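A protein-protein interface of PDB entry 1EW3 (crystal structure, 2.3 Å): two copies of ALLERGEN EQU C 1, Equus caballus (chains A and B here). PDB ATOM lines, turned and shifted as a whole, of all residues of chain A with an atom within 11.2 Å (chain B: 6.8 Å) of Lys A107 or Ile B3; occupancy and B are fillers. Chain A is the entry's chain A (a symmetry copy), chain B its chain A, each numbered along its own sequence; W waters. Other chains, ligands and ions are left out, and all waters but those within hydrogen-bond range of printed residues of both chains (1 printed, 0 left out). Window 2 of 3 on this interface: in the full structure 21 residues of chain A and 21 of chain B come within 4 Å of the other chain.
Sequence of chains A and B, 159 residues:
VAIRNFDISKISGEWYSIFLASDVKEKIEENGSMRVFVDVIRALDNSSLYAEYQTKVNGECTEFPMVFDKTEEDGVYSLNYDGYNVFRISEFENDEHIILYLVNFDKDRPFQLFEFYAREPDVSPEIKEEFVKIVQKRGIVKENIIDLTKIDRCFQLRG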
ATOM      1  N   VAL A  24       1.898  17.786  -3.547  1.00  0.00           N
ATOM      2  CA  VAL A  24       3.285  17.592  -3.973  1.00  0.00           C
ATOM      3  C   VAL A  24       3.340  16.214  -4.632  1.00  0.00           C
ATOM      4  O   VAL A  24       3.558  15.143  -4.039  1.00  0.00           O
ATOM      5  CB  VAL A  24       4.256  17.738  -2.821  1.00  0.00           C
ATOM      6  CG1 VAL A  24       5.690  17.453  -3.266  1.00  0.00           C
ATOM      7  CG2 VAL A  24       4.166  19.097  -2.140  1.00  0.00           C
ATOM      8  N   LYS A  27       5.473  12.923  -4.350  1.00  0.00           N
ATOM      9  CA  LYS A  27       5.330  12.030  -3.208  1.00  0.00           C
ATOM     10  C   LYS A  27       4.441  10.869  -3.612  1.00  0.00           C
ATOM     11  O   LYS A  27       4.644   9.824  -2.991  1.00  0.00           O
ATOM     12  CB  LYS A  27       4.733  12.842  -2.046  1.00  0.00           C
ATOM     13  CG  LYS A  27       5.753  13.826  -1.430  1.00  0.00           C
ATOM     14  CD  LYS A  27       6.864  12.951  -0.855  1.00  0.00           C
ATOM     15  CE  LYS A  27       8.035  13.706  -0.310  1.00  0.00           C
ATOM     16  NZ  LYS A  27       9.125  12.782   0.142  1.00  0.00           N
ATOM     17  N   ASP A  82       9.125   8.969   6.667  1.00  0.00           N
ATOM     18  CA  ASP A  82       9.577   9.988   5.750  1.00  0.00           C
ATOM     19  C   ASP A  82       9.384  11.385   6.361  1.00  0.00           C
ATOM     20  O   ASP A  82       8.702  12.242   5.807  1.00  0.00           O
ATOM     21  CB  ASP A  82       8.770   9.901   4.447  1.00  0.00           C
ATOM     22  CG  ASP A  82       9.376  10.845   3.408  1.00  0.00           C
ATOM     23  OD1 ASP A  82      10.542  11.240   3.610  1.00  0.00           O
ATOM     24  OD2 ASP A  82       8.692  11.209   2.445  1.00  0.00           O
ATOM     25  N   GLY A  83       9.692  11.505   7.625  1.00  0.00           N
ATOM     26  CA  GLY A  83       9.562  12.484   8.621  1.00  0.00           C
ATOM     27  C   GLY A  83       8.319  12.268   9.509  1.00  0.00           C
ATOM     28  O   GLY A  83       7.764  11.167   9.701  1.00  0.00           O
ATOM     29  N   TYR A  84       7.808  13.383  10.065  1.00  0.00           N
ATOM     30  CA  TYR A  84       6.686  13.328  11.006  1.00  0.00           C
ATOM     31  C   TYR A  84       5.372  13.682  10.339  1.00  0.00           C
ATOM     32  O   TYR A  84       5.294  14.725   9.691  1.00  0.00           O
ATOM     33  CB  TYR A  84       7.023  14.276  12.140  1.00  0.00           C
ATOM     34  CG  TYR A  84       6.020  14.212  13.264  1.00  0.00           C
ATOM     35  CD1 TYR A  84       5.971  13.125  14.143  1.00  0.00           C
ATOM     36  CD2 TYR A  84       5.124  15.266  13.400  1.00  0.00           C
ATOM     37  CE1 TYR A  84       5.014  13.074  15.128  1.00  0.00           C
ATOM     38  CE2 TYR A  84       4.208  15.235  14.424  1.00  0.00           C
ATOM     39  CZ  TYR A  84       4.171  14.158  15.294  1.00  0.00           C
ATOM     40  OH  TYR A  84       3.177  14.175  16.255  1.00  0.00           O
ATOM     41  N   ASN A  85       4.338  12.904  10.507  1.00  0.00           N
ATOM     42  CA  ASN A  85       3.067  13.044   9.860  1.00  0.00           C
ATOM     43  C   ASN A  85       1.933  13.040  10.893  1.00  0.00           C
ATOM     44  O   ASN A  85       2.024  12.260  11.825  1.00  0.00           O
ATOM     45  CB  ASN A  85       2.807  11.775   8.952  1.00  0.00           C
ATOM     46  CG  ASN A  85       3.956  11.587   7.968  1.00  0.00           C
ATOM     47  OD1 ASN A  85       4.024  12.203   6.892  1.00  0.00           O
ATOM     48  ND2 ASN A  85       4.962  10.786   8.327  1.00  0.00           N
ATOM     49  N   VAL A 103      -0.828  15.338   6.827  1.00  0.00           N
ATOM     50  CA  VAL A 103       0.121  16.358   6.574  1.00  0.00           C
ATOM     51  C   VAL A 103       1.452  15.840   7.087  1.00  0.00           C
ATOM     52  O   VAL A 103       1.481  15.246   8.152  1.00  0.00           O
ATOM     53  CB  VAL A 103      -0.247  17.713   7.261  1.00  0.00           C
ATOM     54  CG1 VAL A 103       0.836  18.736   7.124  1.00  0.00           C
ATOM     55  CG2 VAL A 103      -1.561  18.225   6.731  1.00  0.00           C
ATOM     56  N   ASN A 104       2.505  16.106   6.358  1.00  0.00           N
ATOM     57  CA  ASN A 104       3.871  15.791   6.694  1.00  0.00           C
ATOM     58  C   ASN A 104       4.494  17.164   6.967  1.00  0.00           C
ATOM     59  O   ASN A 104       4.538  18.065   6.120  1.00  0.00           O
ATOM     60  CB  ASN A 104       4.478  15.118   5.418  1.00  0.00           C
ATOM     61  CG  ASN A 104       5.912  14.724   5.662  1.00  0.00           C
ATOM     62  OD1 ASN A 104       6.776  15.564   5.774  1.00  0.00           O
ATOM     63  ND2 ASN A 104       6.197  13.430   5.790  1.00  0.00           N
ATOM     64  N   PHE A 105       5.053  17.300   8.153  1.00  0.00           N
ATOM     65  CA  PHE A 105       5.609  18.506   8.688  1.00  0.00           C
ATOM     66  C   PHE A 105       7.075  18.647   8.381  1.00  0.00           C
ATOM     67  O   PHE A 105       7.817  19.262   9.131  1.00  0.00           O
ATOM     68  CB  PHE A 105       5.324  18.686  10.200  1.00  0.00           C
ATOM     69  CG  PHE A 105       3.864  18.991  10.450  1.00  0.00           C
ATOM     70  CD1 PHE A 105       2.928  17.998  10.578  1.00  0.00           C
ATOM     71  CD2 PHE A 105       3.441  20.323  10.527  1.00  0.00           C
ATOM     72  CE1 PHE A 105       1.581  18.288  10.776  1.00  0.00           C
ATOM     73  CE2 PHE A 105       2.097  20.625  10.748  1.00  0.00           C
ATOM     74  CZ  PHE A 105       1.160  19.638  10.852  1.00  0.00           C
ATOM     75  N   ASP A 106       7.429  18.253   7.155  1.00  0.00           N
ATOM     76  CA  ASP A 106       8.826  18.492   6.727  1.00  0.00           C
ATOM     77  C   ASP A 106       9.076  19.988   6.747  1.00  0.00           C
ATOM     78  O   ASP A 106       8.234  20.808   6.353  1.00  0.00           O
ATOM     79  CB  ASP A 106       8.999  17.918   5.317  1.00  0.00           C
ATOM     80  CG  ASP A 106      10.417  18.187   4.828  1.00  0.00           C
ATOM     81  OD1 ASP A 106      11.389  17.595   5.329  1.00  0.00           O
ATOM     82  OD2 ASP A 106      10.545  19.026   3.931  1.00  0.00           O
ATOM     83  N   LYS A 107      10.201  20.382   7.288  1.00  0.00           N
ATOM     84  CA  LYS A 107      10.555  21.790   7.410  1.00  0.00           C
ATOM     85  C   LYS A 107      10.548  22.515   6.059  1.00  0.00           C
ATOM     86  O   LYS A 107       9.913  23.553   5.852  1.00  0.00           O
ATOM     87  CB  LYS A 107      11.976  21.843   8.006  1.00  0.00           C
ATOM     88  CG  LYS A 107      12.583  23.219   7.940  1.00  0.00           C
ATOM     89  CD  LYS A 107      13.845  23.376   8.770  1.00  0.00           C
ATOM     90  CE  LYS A 107      15.040  22.727   8.095  1.00  0.00           C
ATOM     91  NZ  LYS A 107      15.448  23.381   6.818  1.00  0.00           N
ATOM     92  N   ASP A 108      11.287  21.925   5.108  1.00  0.00           N
ATOM     93  CA  ASP A 108      11.421  22.570   3.797  1.00  0.00           C
ATOM     94  C   ASP A 108      10.290  22.346   2.836  1.00  0.00           C
ATOM     95  O   ASP A 108       9.888  23.306   2.188  1.00  0.00           O
ATOM     96  CB  ASP A 108      12.795  22.188   3.193  1.00  0.00           C
ATOM     97  CG  ASP A 108      13.775  22.785   4.205  1.00  0.00           C
ATOM     98  OD1 ASP A 108      13.896  24.028   4.186  1.00  0.00           O
ATOM     99  OD2 ASP A 108      14.342  22.081   5.038  1.00  0.00           O
ATOM    100  N   ARG A 109       9.674  21.174   2.829  1.00  0.00           N
ATOM    101  CA  ARG A 109       8.600  20.911   1.891  1.00  0.00           C
ATOM    102  C   ARG A 109       7.481  20.066   2.494  1.00  0.00           C
ATOM    103  O   ARG A 109       7.402  18.875   2.201  1.00  0.00           O
ATOM    104  CB  ARG A 109       9.225  20.180   0.698  1.00  0.00           C
ATOM    105  N   PRO A 110       6.609  20.691   3.279  1.00  0.00           N
ATOM    106  CA  PRO A 110       5.508  19.989   3.906  1.00  0.00           C
ATOM    107  C   PRO A 110       4.500  19.685   2.819  1.00  0.00           C
ATOM    108  O   PRO A 110       4.583  20.358   1.780  1.00  0.00           O
ATOM    109  CB  PRO A 110       4.934  20.976   4.919  1.00  0.00           C
ATOM    110  CG  PRO A 110       5.320  22.304   4.349  1.00  0.00           C
ATOM    111  CD  PRO A 110       6.668  22.118   3.710  1.00  0.00           C
ATOM    112  N   PHE A 111       3.572  18.747   3.076  1.00  0.00           N
ATOM    113  CA  PHE A 111       2.561  18.630   2.020  1.00  0.00           C
ATOM    114  C   PHE A 111       1.347  17.989   2.655  1.00  0.00           C
ATOM    115  O   PHE A 111       1.478  17.433   3.748  1.00  0.00           O
ATOM    116  CB  PHE A 111       3.117  17.669   0.948  1.00  0.00           C
ATOM    117  CG  PHE A 111       3.563  16.301   1.376  1.00  0.00           C
ATOM    118  CD1 PHE A 111       2.689  15.237   1.461  1.00  0.00           C
ATOM    119  CD2 PHE A 111       4.882  16.060   1.671  1.00  0.00           C
ATOM    120  CE1 PHE A 111       3.128  13.958   1.780  1.00  0.00           C
ATOM    121  CE2 PHE A 111       5.342  14.805   1.997  1.00  0.00           C
ATOM    122  CZ  PHE A 111       4.449  13.747   2.042  1.00  0.00           C
ATOM    123  N   VAL B   1      15.491  32.922   2.534  1.00  0.00           N
ATOM    124  CA  VAL B   1      15.638  31.535   1.999  1.00  0.00           C
ATOM    125  C   VAL B   1      15.944  30.561   3.143  1.00  0.00           C
ATOM    126  O   VAL B   1      15.438  29.443   3.181  1.00  0.00           O
ATOM    127  CB  VAL B   1      16.839  31.438   1.035  1.00  0.00           C
ATOM    128  CG1 VAL B   1      16.559  30.497  -0.127  1.00  0.00           C
ATOM    129  CG2 VAL B   1      17.271  32.829   0.609  1.00  0.00           C
ATOM    130  N   ALA B   2      16.773  31.040   4.049  1.00  0.00           N
ATOM    131  CA  ALA B   2      17.261  30.310   5.199  1.00  0.00           C
ATOM    132  C   ALA B   2      16.206  30.072   6.277  1.00  0.00           C
ATOM    133  O   ALA B   2      15.933  30.900   7.138  1.00  0.00           O
ATOM    134  CB  ALA B   2      18.479  31.066   5.735  1.00  0.00           C
ATOM    135  N   ILE B   3      15.587  28.898   6.238  1.00  0.00           N
ATOM    136  CA  ILE B   3      14.542  28.437   7.125  1.00  0.00           C
ATOM    137  C   ILE B   3      15.069  27.236   7.909  1.00  0.00           C
ATOM    138  O   ILE B   3      15.273  26.171   7.320  1.00  0.00           O
ATOM    139  CB  ILE B   3      13.297  27.975   6.353  1.00  0.00           C
ATOM    140  CG1 ILE B   3      12.468  29.180   5.895  1.00  0.00           C
ATOM    141  CG2 ILE B   3      12.490  27.018   7.195  1.00  0.00           C
ATOM    142  CD1 ILE B   3      11.355  28.832   4.933  1.00  0.00           C
ATOM    143  N   ARG B   4      15.319  27.447   9.194  1.00  0.00           N
ATOM    144  CA  ARG B   4      15.959  26.439   9.995  1.00  0.00           C
ATOM    145  C   ARG B   4      15.153  26.220  11.265  1.00  0.00           C
ATOM    146  O   ARG B   4      14.210  26.947  11.479  1.00  0.00           O
ATOM    147  CB  ARG B   4      17.356  26.897  10.429  1.00  0.00           C
ATOM    148  CG  ARG B   4      18.099  27.803   9.464  1.00  0.00           C
ATOM    149  CD  ARG B   4      19.592  27.795   9.779  1.00  0.00           C
ATOM    150  NE  ARG B   4      20.412  28.421   8.755  1.00  0.00           N
ATOM    151  CZ  ARG B   4      21.624  27.986   8.399  1.00  0.00           C
ATOM    152  NH1 ARG B   4      22.160  26.909   8.976  1.00  0.00           N
ATOM    153  NH2 ARG B   4      22.315  28.621   7.457  1.00  0.00           N
ATOM    154  N   ASN B   5      15.642  25.314  12.088  1.00  0.00           N
ATOM    155  CA  ASN B   5      14.969  25.060  13.361  1.00  0.00           C
ATOM    156  C   ASN B   5      15.311  26.186  14.340  1.00  0.00           C
ATOM    157  O   ASN B   5      16.418  26.732  14.350  1.00  0.00           O
ATOM    158  CB  ASN B   5      15.289  23.672  13.906  1.00  0.00           C
ATOM    159  CG  ASN B   5      14.464  22.632  13.161  1.00  0.00           C
ATOM    160  OD1 ASN B   5      13.326  22.331  13.516  1.00  0.00           O
ATOM    161  ND2 ASN B   5      15.025  22.081  12.087  1.00  0.00           N
ATOM    162  N   GLU B  73       8.529  15.216  17.501  1.00  0.00           N
ATOM    163  CA  GLU B  73       9.354  15.836  16.423  1.00  0.00           C
ATOM    164  C   GLU B  73       9.789  17.236  16.838  1.00  0.00           C
ATOM    165  O   GLU B  73       8.966  18.021  17.362  1.00  0.00           O
ATOM    166  CB  GLU B  73       8.440  15.948  15.178  1.00  0.00           C
ATOM    167  CG  GLU B  73       9.118  16.673  14.038  1.00  0.00           C
ATOM    168  CD  GLU B  73      10.262  15.867  13.462  1.00  0.00           C
ATOM    169  OE1 GLU B  73      11.055  16.445  12.692  1.00  0.00           O
ATOM    170  OE2 GLU B  73      10.337  14.667  13.770  1.00  0.00           O
ATOM    171  N   ARG B  88       4.703  23.699  13.108  1.00  0.00           N
ATOM    172  CA  ARG B  88       6.139  23.765  13.262  1.00  0.00           C
ATOM    173  C   ARG B  88       6.524  25.245  13.359  1.00  0.00           C
ATOM    174  O   ARG B  88       5.977  26.075  12.603  1.00  0.00           O
ATOM    175  CB  ARG B  88       6.864  23.197  11.984  1.00  0.00           C
ATOM    176  CG  ARG B  88       8.378  23.405  12.035  1.00  0.00           C
ATOM    177  CD  ARG B  88       9.015  22.859  10.729  1.00  0.00           C
ATOM    178  NE  ARG B  88       8.809  21.387  10.634  1.00  0.00           N
ATOM    179  CZ  ARG B  88       9.727  20.600  11.232  1.00  0.00           C
ATOM    180  NH1 ARG B  88      10.746  21.139  11.885  1.00  0.00           N
ATOM    181  NH2 ARG B  88       9.681  19.285  11.236  1.00  0.00           N
ATOM    182  N   SER B  90       9.658  27.778  12.799  1.00  0.00           N
ATOM    183  CA  SER B  90      11.010  27.765  12.278  1.00  0.00           C
ATOM    184  C   SER B  90      11.550  29.179  12.411  1.00  0.00           C
ATOM    185  O   SER B  90      10.840  30.145  12.228  1.00  0.00           O
ATOM    186  CB  SER B  90      11.187  27.260  10.837  1.00  0.00           C
ATOM    187  OG  SER B  90      10.278  26.215  10.518  1.00  0.00           O
ATOM    188  N   GLU B  91      12.858  29.284  12.439  1.00  0.00           N
ATOM    189  CA  GLU B  91      13.547  30.571  12.377  1.00  0.00           C
ATOM    190  C   GLU B  91      13.548  30.997  10.919  1.00  0.00           C
ATOM    191  O   GLU B  91      13.637  30.150  10.011  1.00  0.00           O
ATOM    192  CB  GLU B  91      14.895  30.349  13.029  1.00  0.00           C
ATOM    193  CG  GLU B  91      16.131  30.689  12.287  1.00  0.00           C
ATOM    194  CD  GLU B  91      17.359  30.959  13.142  1.00  0.00           C
ATOM    195  OE1 GLU B  91      17.523  30.592  14.323  1.00  0.00           O
ATOM    196  OE2 GLU B  91      18.214  31.614  12.535  1.00  0.00           O
ATOM    197  N   PHE B  92      13.237  32.277  10.660  1.00  0.00           N
ATOM    198  CA  PHE B  92      13.223  32.734   9.252  1.00  0.00           C
ATOM    199  C   PHE B  92      14.324  33.754   9.032  1.00  0.00           C
ATOM    200  O   PHE B  92      14.369  34.892   9.522  1.00  0.00           O
ATOM    201  CB  PHE B  92      11.858  33.261   8.931  1.00  0.00           C
ATOM    202  CG  PHE B  92      11.533  33.715   7.554  1.00  0.00           C
ATOM    203  CD1 PHE B  92      10.843  32.908   6.681  1.00  0.00           C
ATOM    204  CD2 PHE B  92      11.864  34.992   7.130  1.00  0.00           C
ATOM    205  CE1 PHE B  92      10.497  33.332   5.412  1.00  0.00           C
ATOM    206  CE2 PHE B  92      11.522  35.430   5.859  1.00  0.00           C
ATOM    207  CZ  PHE B  92      10.843  34.596   5.002  1.00  0.00           C
ATOM    208  N   GLU B  93      15.344  33.286   8.337  1.00  0.00           N
ATOM    209  CA  GLU B  93      16.539  34.007   7.979  1.00  0.00           C
ATOM    210  C   GLU B  93      17.445  34.260   9.168  1.00  0.00           C
ATOM    211  O   GLU B  93      18.653  34.247   8.950  1.00  0.00           O
ATOM    212  CB  GLU B  93      16.248  35.305   7.229  1.00  0.00           C
ATOM    213  CG  GLU B  93      17.520  35.859   6.581  1.00  0.00           C
ATOM    214  CD  GLU B  93      18.120  34.777   5.668  1.00  0.00           C
ATOM    215  OE1 GLU B  93      17.388  34.450   4.697  1.00  0.00           O
ATOM    216  OE2 GLU B  93      19.243  34.301   5.964  1.00  0.00           O
ATOM    217  N   ILE B  99       8.798  31.911  11.429  1.00  0.00           N
ATOM    218  CA  ILE B  99       7.773  31.492  10.488  1.00  0.00           C
ATOM    219  C   ILE B  99       7.087  30.270  11.107  1.00  0.00           C
ATOM    220  O   ILE B  99       7.707  29.333  11.575  1.00  0.00           O
ATOM    221  CB  ILE B  99       8.232  31.256   9.053  1.00  0.00           C
ATOM    222  CG1 ILE B  99       6.978  30.964   8.213  1.00  0.00           C
ATOM    223  CG2 ILE B  99       9.288  30.169   8.901  1.00  0.00           C
ATOM    224  CD1 ILE B  99       7.232  31.320   6.744  1.00  0.00           C
ATOM    225  N   GLU B 130       9.923  37.612   0.509  1.00  0.00           N
ATOM    226  CA  GLU B 130      10.267  36.219   0.781  1.00  0.00           C
ATOM    227  C   GLU B 130       9.138  35.494   1.486  1.00  0.00           C
ATOM    228  O   GLU B 130       8.758  34.375   1.124  1.00  0.00           O
ATOM    229  CB  GLU B 130      11.553  36.164   1.615  1.00  0.00           C
ATOM    230  CG  GLU B 130      12.366  34.874   1.467  1.00  0.00           C
ATOM    231  CD  GLU B 130      12.220  34.136   0.140  1.00  0.00           C
ATOM    232  OE1 GLU B 130      12.775  34.641  -0.869  1.00  0.00           O
ATOM    233  OE2 GLU B 130      11.536  33.081   0.066  1.00  0.00           O
ATOM    234  N   ILE B 134       7.085  32.131  -0.159  1.00  0.00           N
ATOM    235  CA  ILE B 134       6.954  30.899   0.599  1.00  0.00           C
ATOM    236  C   ILE B 134       5.527  30.467   0.759  1.00  0.00           C
ATOM    237  O   ILE B 134       5.221  29.310   0.512  1.00  0.00           O
ATOM    238  CB  ILE B 134       7.585  30.968   1.996  1.00  0.00           C
ATOM    239  CG1 ILE B 134       9.098  30.883   1.842  1.00  0.00           C
ATOM    240  CG2 ILE B 134       7.018  29.827   2.843  1.00  0.00           C
ATOM    241  CD1 ILE B 134       9.782  31.664   2.941  1.00  0.00           C
HETATM  242  O   HOH W   1       6.732  22.344   8.260  1.00  0.00           O
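O of Ile B3 lies within hydrogen-bond range of NZ of Lys A107, 2.8 Å away. NE of Arg B88 lies within hydrogen-bond range of O of Phe A105 (2.8 Å).
The side-chain amino group (NZ) of Lys A107 lies within salt-bridge range of the side-chain carboxylate (OD2) of Asp A108, at 2.5 Å. The side-chain carboxylate (OE1) of Glu B73 is in salt-bridge range of the guanidinium group (NH2) of Arg B88, 3.5 Å away. The backbone carbonyl oxygen (O) of Tyr A84 lies within hydrogen-bond range of the backbone NH (N) of Phe A105 (3.0 Å). NH1 of Arg B88 is in hydrogen-bond range of OD1 of Asn B5 (3.3 Å). O of Arg B4 lies within hydrogen-bond range of N of Glu B91, at 2.9 Å.
Among the printed residues, merely in contact across the chains: Tyr A84 with Glu B73, Lys A107 with Arg B4, Lys A107 with Asn B5 and Lys A107 with Arg B88.
Of the printed residues of chain A, Ile B3 touches Lys A107. No residue of chain A comes within 4 Å of Ala B2. Of chain A, only Lys A107 (3.8 Å) comes within 4 Å of Asn B5. Printed residues of chain A within 4 Å of Glu B73: Tyr A84 (3.5 Å). Printed residues of chain B within 4 Å of Tyr A84: Glu B73. Printed residues of chain B within 4 Å of Phe A105: Arg B88 (2.8 Å). Printed residues of chain A within 4 Å of Arg B88: Phe A105 (2.8 Å) and Lys A107 (3.7 Å). The nearest residue of chain B that does not touch Lys A107 is Ser B90 (4.6 Å). The nearest residue of chain A that does not touch Ile B3 is Asp A108 (4.04 Å). The nearest printed residue of chain A that does not touch Arg B88 is Asp A106 (4.1 Å).
Of the 14 printed residues of chain B, 5 touch a printed residue of chain A. Printed residues of chain B that touch a printed residue of chain A: Ile B3, Arg B4, Asn B5, Glu B73 and Arg B88. Hydrophobic or aromatic side chains of chain B that line the printed part of chain A: Ile B3. Among the printed residues, 6 pairs touch across the chains. Among the printed residues, no Asp or Glu carboxylate lies within 4 Å of a Lys or Arg side-chain nitrogen of the other chain.
No position is printed for both chains.
Water W1 lies within hydrogen-bond range of the backbone carbonyl oxygen of Asp A106 (2.9 Å), the guanidinium group of Arg B88 (3.3 Å) and the backbone carbonyl oxygen of Phe A105 (3.4 Å).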
